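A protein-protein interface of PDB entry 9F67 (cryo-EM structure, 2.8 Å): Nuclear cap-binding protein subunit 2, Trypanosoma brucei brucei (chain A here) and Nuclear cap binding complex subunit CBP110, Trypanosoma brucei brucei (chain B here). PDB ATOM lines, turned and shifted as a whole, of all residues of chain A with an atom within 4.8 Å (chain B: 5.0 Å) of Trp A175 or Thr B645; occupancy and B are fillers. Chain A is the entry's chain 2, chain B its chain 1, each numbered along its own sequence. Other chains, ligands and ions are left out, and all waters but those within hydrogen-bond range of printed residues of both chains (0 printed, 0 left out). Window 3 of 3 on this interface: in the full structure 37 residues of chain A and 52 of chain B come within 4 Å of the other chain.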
ATOM      1  N   GLU A  55     -13.732   3.609 -22.576  1.00  0.00           N
ATOM      2  CA  GLU A  55     -14.540   4.398 -21.605  1.00  0.00           C
ATOM      3  C   GLU A  55     -13.997   5.824 -21.480  1.00  0.00           C
ATOM      4  O   GLU A  55     -14.822   6.723 -21.312  1.00  0.00           O
ATOM      5  CB  GLU A  55     -14.587   3.745 -20.223  1.00  0.00           C
ATOM      6  CG  GLU A  55     -15.326   2.423 -20.185  1.00  0.00           C
ATOM      7  CD  GLU A  55     -15.486   1.881 -18.775  1.00  0.00           C
ATOM      8  OE1 GLU A  55     -15.018   2.550 -17.836  1.00  0.00           O
ATOM      9  OE2 GLU A  55     -16.090   0.803 -18.617  1.00  0.00           O
ATOM     10  N   ASP A  56     -12.679   6.034 -21.509  1.00  0.00           N
ATOM     11  CA  ASP A  56     -12.198   7.428 -21.307  1.00  0.00           C
ATOM     12  C   ASP A  56     -12.748   8.322 -22.423  1.00  0.00           C
ATOM     13  O   ASP A  56     -13.175   9.444 -22.105  1.00  0.00           O
ATOM     14  CB  ASP A  56     -10.673   7.535 -21.259  1.00  0.00           C
ATOM     15  CG  ASP A  56     -10.049   6.806 -20.085  1.00  0.00           C
ATOM     16  OD1 ASP A  56     -10.805   6.194 -19.305  1.00  0.00           O
ATOM     17  OD2 ASP A  56      -8.815   6.897 -19.943  1.00  0.00           O
ATOM     18  N   ARG A  80     -16.118 -11.076 -21.863  1.00  0.00           N
ATOM     19  CA  ARG A  80     -15.876  -9.987 -20.872  1.00  0.00           C
ATOM     20  C   ARG A  80     -15.146  -8.844 -21.592  1.00  0.00           C
ATOM     21  O   ARG A  80     -14.223  -8.262 -20.986  1.00  0.00           O
ATOM     22  CB  ARG A  80     -15.160 -10.566 -19.645  1.00  0.00           C
ATOM     23  CG  ARG A  80     -15.972 -11.660 -18.967  1.00  0.00           C
ATOM     24  CD  ARG A  80     -15.323 -12.442 -17.841  1.00  0.00           C
ATOM     25  NE  ARG A  80     -14.879 -11.715 -16.663  1.00  0.00           N
ATOM     26  CZ  ARG A  80     -13.621 -11.691 -16.239  1.00  0.00           C
ATOM     27  NH1 ARG A  80     -12.659 -12.184 -16.997  1.00  0.00           N
ATOM     28  NH2 ARG A  80     -13.327 -11.161 -15.065  1.00  0.00           N
ATOM     29  N   TYR A 173     -11.879  -6.825 -19.758  1.00  0.00           N
ATOM     30  CA  TYR A 173     -12.259  -6.315 -18.439  1.00  0.00           C
ATOM     31  C   TYR A 173     -12.299  -7.509 -17.516  1.00  0.00           C
ATOM     32  O   TYR A 173     -13.343  -8.088 -17.355  1.00  0.00           O
ATOM     33  CB  TYR A 173     -13.570  -5.564 -18.499  1.00  0.00           C
ATOM     34  CG  TYR A 173     -13.651  -4.212 -19.148  1.00  0.00           C
ATOM     35  CD1 TYR A 173     -13.303  -4.011 -20.464  1.00  0.00           C
ATOM     36  CD2 TYR A 173     -14.204  -3.151 -18.462  1.00  0.00           C
ATOM     37  CE1 TYR A 173     -13.423  -2.769 -21.055  1.00  0.00           C
ATOM     38  CE2 TYR A 173     -14.335  -1.903 -19.034  1.00  0.00           C
ATOM     39  CZ  TYR A 173     -13.934  -1.711 -20.336  1.00  0.00           C
ATOM     40  OH  TYR A 173     -14.059  -0.483 -20.927  1.00  0.00           O
ATOM     41  N   THR A 174     -11.196  -7.813 -16.885  1.00  0.00           N
ATOM     42  CA  THR A 174     -11.037  -9.004 -16.052  1.00  0.00           C
ATOM     43  C   THR A 174     -11.227  -8.648 -14.600  1.00  0.00           C
ATOM     44  O   THR A 174     -11.038  -9.524 -13.770  1.00  0.00           O
ATOM     45  CB  THR A 174      -9.618  -9.462 -16.302  1.00  0.00           C
ATOM     46  OG1 THR A 174      -8.760  -8.375 -15.972  1.00  0.00           O
ATOM     47  CG2 THR A 174      -9.377  -9.846 -17.743  1.00  0.00           C
ATOM     48  N   TRP A 175     -11.563  -7.385 -14.342  1.00  0.00           N
ATOM     49  CA  TRP A 175     -11.814  -6.922 -12.958  1.00  0.00           C
ATOM     50  C   TRP A 175     -13.322  -6.975 -12.706  1.00  0.00           C
ATOM     51  O   TRP A 175     -13.765  -6.489 -11.646  1.00  0.00           O
ATOM     52  CB  TRP A 175     -11.211  -5.523 -12.784  1.00  0.00           C
ATOM     53  CG  TRP A 175     -11.729  -4.480 -13.726  1.00  0.00           C
ATOM     54  CD1 TRP A 175     -13.009  -4.022 -13.836  1.00  0.00           C
ATOM     55  CD2 TRP A 175     -10.978  -3.796 -14.744  1.00  0.00           C
ATOM     56  NE1 TRP A 175     -13.102  -3.084 -14.828  1.00  0.00           N
ATOM     57  CE2 TRP A 175     -11.872  -2.925 -15.406  1.00  0.00           C
ATOM     58  CE3 TRP A 175      -9.641  -3.825 -15.154  1.00  0.00           C
ATOM     59  CZ2 TRP A 175     -11.468  -2.095 -16.448  1.00  0.00           C
ATOM     60  CZ3 TRP A 175      -9.244  -3.003 -16.185  1.00  0.00           C
ATOM     61  CH2 TRP A 175     -10.145  -2.152 -16.821  1.00  0.00           C
ATOM     62  N   ILE A 176     -14.072  -7.549 -13.655  1.00  0.00           N
ATOM     63  CA  ILE A 176     -15.526  -7.621 -13.503  1.00  0.00           C
ATOM     64  C   ILE A 176     -15.791  -9.094 -13.375  1.00  0.00           C
ATOM     65  O   ILE A 176     -15.425  -9.833 -14.271  1.00  0.00           O
ATOM     66  CB  ILE A 176     -16.179  -6.985 -14.731  1.00  0.00           C
ATOM     67  CG1 ILE A 176     -15.815  -5.510 -14.853  1.00  0.00           C
ATOM     68  CG2 ILE A 176     -17.682  -7.160 -14.679  1.00  0.00           C
ATOM     69  CD1 ILE A 176     -16.284  -4.686 -13.682  1.00  0.00           C
ATOM     70  N   PRO A 177     -16.461  -9.531 -12.310  1.00  0.00           N
ATOM     71  CA  PRO A 177     -16.659 -10.904 -12.094  1.00  0.00           C
ATOM     72  C   PRO A 177     -17.439 -11.558 -13.226  1.00  0.00           C
ATOM     73  O   PRO A 177     -18.364 -10.960 -13.697  1.00  0.00           O
ATOM     74  CB  PRO A 177     -17.671 -10.820 -10.984  1.00  0.00           C
ATOM     75  CG  PRO A 177     -18.260  -9.454 -11.041  1.00  0.00           C
ATOM     76  CD  PRO A 177     -17.019  -8.653 -11.298  1.00  0.00           C
ATOM     77  N   PRO B 564     -10.341  -5.480  -8.356  1.00  0.00           N
ATOM     78  CA  PRO B 564     -11.224  -4.412  -7.861  1.00  0.00           C
ATOM     79  C   PRO B 564     -12.573  -4.909  -7.382  1.00  0.00           C
ATOM     80  O   PRO B 564     -13.185  -4.272  -6.517  1.00  0.00           O
ATOM     81  CB  PRO B 564     -11.364  -3.489  -9.077  1.00  0.00           C
ATOM     82  CG  PRO B 564     -10.140  -3.748  -9.880  1.00  0.00           C
ATOM     83  CD  PRO B 564      -9.834  -5.199  -9.706  1.00  0.00           C
ATOM     84  N   SER B 565     -13.063  -6.022  -7.928  1.00  0.00           N
ATOM     85  CA  SER B 565     -14.310  -6.591  -7.434  1.00  0.00           C
ATOM     86  C   SER B 565     -14.172  -7.067  -5.994  1.00  0.00           C
ATOM     87  O   SER B 565     -15.077  -6.861  -5.177  1.00  0.00           O
ATOM     88  CB  SER B 565     -14.751  -7.742  -8.338  1.00  0.00           C
ATOM     89  OG  SER B 565     -13.887  -8.855  -8.197  1.00  0.00           O
ATOM     90  N   THR B 641      -4.188   0.735 -10.802  1.00  0.00           N
ATOM     91  CA  THR B 641      -5.181   1.125 -11.794  1.00  0.00           C
ATOM     92  C   THR B 641      -4.538   1.773 -13.009  1.00  0.00           C
ATOM     93  O   THR B 641      -5.076   1.671 -14.116  1.00  0.00           O
ATOM     94  CB  THR B 641      -6.202   2.072 -11.171  1.00  0.00           C
ATOM     95  OG1 THR B 641      -5.527   3.214 -10.633  1.00  0.00           O
ATOM     96  CG2 THR B 641      -6.950   1.381 -10.062  1.00  0.00           C
ATOM     97  N   LEU B 643      -4.753   4.549 -13.711  1.00  0.00           N
ATOM     98  CA  LEU B 643      -5.692   5.609 -14.055  1.00  0.00           C
ATOM     99  C   LEU B 643      -6.077   5.551 -15.529  1.00  0.00           C
ATOM    100  O   LEU B 643      -6.281   6.576 -16.182  1.00  0.00           O
ATOM    101  CB  LEU B 643      -5.124   6.976 -13.687  1.00  0.00           C
ATOM    102  CG  LEU B 643      -5.251   7.374 -12.220  1.00  0.00           C
ATOM    103  CD1 LEU B 643      -4.162   6.748 -11.396  1.00  0.00           C
ATOM    104  CD2 LEU B 643      -5.204   8.870 -12.083  1.00  0.00           C
ATOM    105  N   ARG B 644      -6.182   4.336 -16.060  1.00  0.00           N
ATOM    106  CA  ARG B 644      -6.540   4.167 -17.460  1.00  0.00           C
ATOM    107  C   ARG B 644      -8.037   4.024 -17.667  1.00  0.00           C
ATOM    108  O   ARG B 644      -8.550   4.425 -18.717  1.00  0.00           O
ATOM    109  CB  ARG B 644      -5.827   2.949 -18.052  1.00  0.00           C
ATOM    110  CG  ARG B 644      -6.068   1.659 -17.300  1.00  0.00           C
ATOM    111  CD  ARG B 644      -5.407   0.492 -18.004  1.00  0.00           C
ATOM    112  NE  ARG B 644      -3.973   0.448 -17.756  1.00  0.00           N
ATOM    113  CZ  ARG B 644      -3.047   0.698 -18.672  1.00  0.00           C
ATOM    114  NH1 ARG B 644      -3.374   1.019 -19.913  1.00  0.00           N
ATOM    115  NH2 ARG B 644      -1.763   0.625 -18.335  1.00  0.00           N
ATOM    116  N   THR B 645      -8.749   3.462 -16.695  1.00  0.00           N
ATOM    117  CA  THR B 645     -10.191   3.298 -16.774  1.00  0.00           C
ATOM    118  C   THR B 645     -10.838   4.057 -15.627  1.00  0.00           C
ATOM    119  O   THR B 645     -10.448   3.892 -14.468  1.00  0.00           O
ATOM    120  CB  THR B 645     -10.585   1.821 -16.734  1.00  0.00           C
ATOM    121  OG1 THR B 645     -10.146   1.173 -17.931  1.00  0.00           O
ATOM    122  CG2 THR B 645     -12.084   1.674 -16.614  1.00  0.00           C
ATOM    123  N   VAL B 646     -11.817   4.897 -15.959  1.00  0.00           N
ATOM    124  CA  VAL B 646     -12.503   5.684 -14.941  1.00  0.00           C
ATOM    125  C   VAL B 646     -13.297   4.783 -14.011  1.00  0.00           C
ATOM    126  O   VAL B 646     -13.407   5.053 -12.808  1.00  0.00           O
ATOM    127  CB  VAL B 646     -13.405   6.735 -15.605  1.00  0.00           C
ATOM    128  CG1 VAL B 646     -13.686   7.859 -14.644  1.00  0.00           C
ATOM    129  CG2 VAL B 646     -12.755   7.263 -16.872  1.00  0.00           C
ATOM    130  N   SER B 647     -13.871   3.705 -14.546  1.00  0.00           N
ATOM    131  CA  SER B 647     -14.737   2.852 -13.745  1.00  0.00           C
ATOM    132  C   SER B 647     -13.973   2.211 -12.595  1.00  0.00           C
ATOM    133  O   SER B 647     -14.435   2.219 -11.449  1.00  0.00           O
ATOM    134  CB  SER B 647     -15.381   1.785 -14.628  1.00  0.00           C
ATOM    135  OG  SER B 647     -14.518   0.676 -14.802  1.00  0.00           O
ATOM    136  N   VAL B 648     -12.792   1.658 -12.877  1.00  0.00           N
ATOM    137  CA  VAL B 648     -12.045   0.968 -11.832  1.00  0.00           C
ATOM    138  C   VAL B 648     -11.521   1.961 -10.803  1.00  0.00           C
ATOM    139  O   VAL B 648     -11.529   1.684  -9.597  1.00  0.00           O
ATOM    140  CB  VAL B 648     -10.918   0.116 -12.442  1.00  0.00           C
ATOM    141  CG1 VAL B 648     -10.043   0.943 -13.343  1.00  0.00           C
ATOM    142  CG2 VAL B 648     -10.089  -0.517 -11.351  1.00  0.00           C
ATOM    143  N   VAL B 649     -11.077   3.133 -11.254  1.00  0.00           N
ATOM    144  CA  VAL B 649     -10.577   4.143 -10.325  1.00  0.00           C
ATOM    145  C   VAL B 649     -11.691   4.599  -9.396  1.00  0.00           C
ATOM    146  O   VAL B 649     -11.505   4.698  -8.176  1.00  0.00           O
ATOM    147  CB  VAL B 649      -9.964   5.326 -11.094  1.00  0.00           C
ATOM    148  CG1 VAL B 649      -9.667   6.463 -10.150  1.00  0.00           C
ATOM    149  CG2 VAL B 649      -8.702   4.891 -11.808  1.00  0.00           C
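The side-chain carboxylate (OD2) of Asp A56 sits close to the backbone carbonyl oxygen (O) of Arg B644, 2.8 Å away.
The side-chain hydroxyl (OH) of Tyr A173 sits close to the side-chain carboxylate (OE2) of Glu A55 (3.3 Å).
Among the printed residues, merely in contact across the chains: Glu A55 with Thr B645 (3.3 Å), Glu A55 with Ser B647 (3.3 Å), Asp A56 with Thr B645 (3.9 Å), Asp A56 with Val B646 (3.3 Å), Trp A175 with Pro B564 (3.4 Å), Trp A175 with Ser B565 (3.7 Å), Trp A175 with Thr B645 (3.5 Å) and Pro A177 with Ser B565 (3.8 Å).
Of the printed residues of chain B, Glu A55 touches Thr B645 (3.3 Å) and Ser B647 (3.3 Å). Tyr A173 touches none of the printed residues of chain B. Printed residues of chain A within 4 Å of Ser B565: Trp A175 (3.7 Å) and Pro A177 (3.8 Å). Of the printed residues of chain A, Thr B645 touches Glu A55 (3.3 Å), Asp A56 (3.9 Å) and Trp A175 (3.5 Å). Of the printed residues of chain A, Val B646 touches Asp A56. Of the printed residues of chain A, Ser B647 touches Glu A55 (3.3 Å). The nearest printed residue of chain B that does not touch Trp A175 is Ser B647 (4.02 Å). The nearest printed residue of chain A that does not touch Thr B645 is Tyr A173 (4.9 Å). The nearest printed residue of chain A that does not touch Ser B565 is Ile A176 (5.2 Å).
Of the 10 printed residues of chain B, 6 touch a printed residue of chain A. Printed residues of chain B that touch a printed residue of chain A: Pro B564, Ser B565, Arg B644, Thr B645, Val B646 and Ser B647. Hydrophobic or aromatic side chains of chain B within 4 Å of the printed part of chain A: Pro B564 and Val B646. Of the 8 printed residues of chain A, 4 touch a printed residue of chain B. Printed residues of chain A that touch a printed residue of chain B: Glu A55, Asp A56, Trp A175 and Pro A177. Hydrophobic or aromatic side chains of chain A within 4 Å of the printed part of chain B: Trp A175 and Pro A177.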
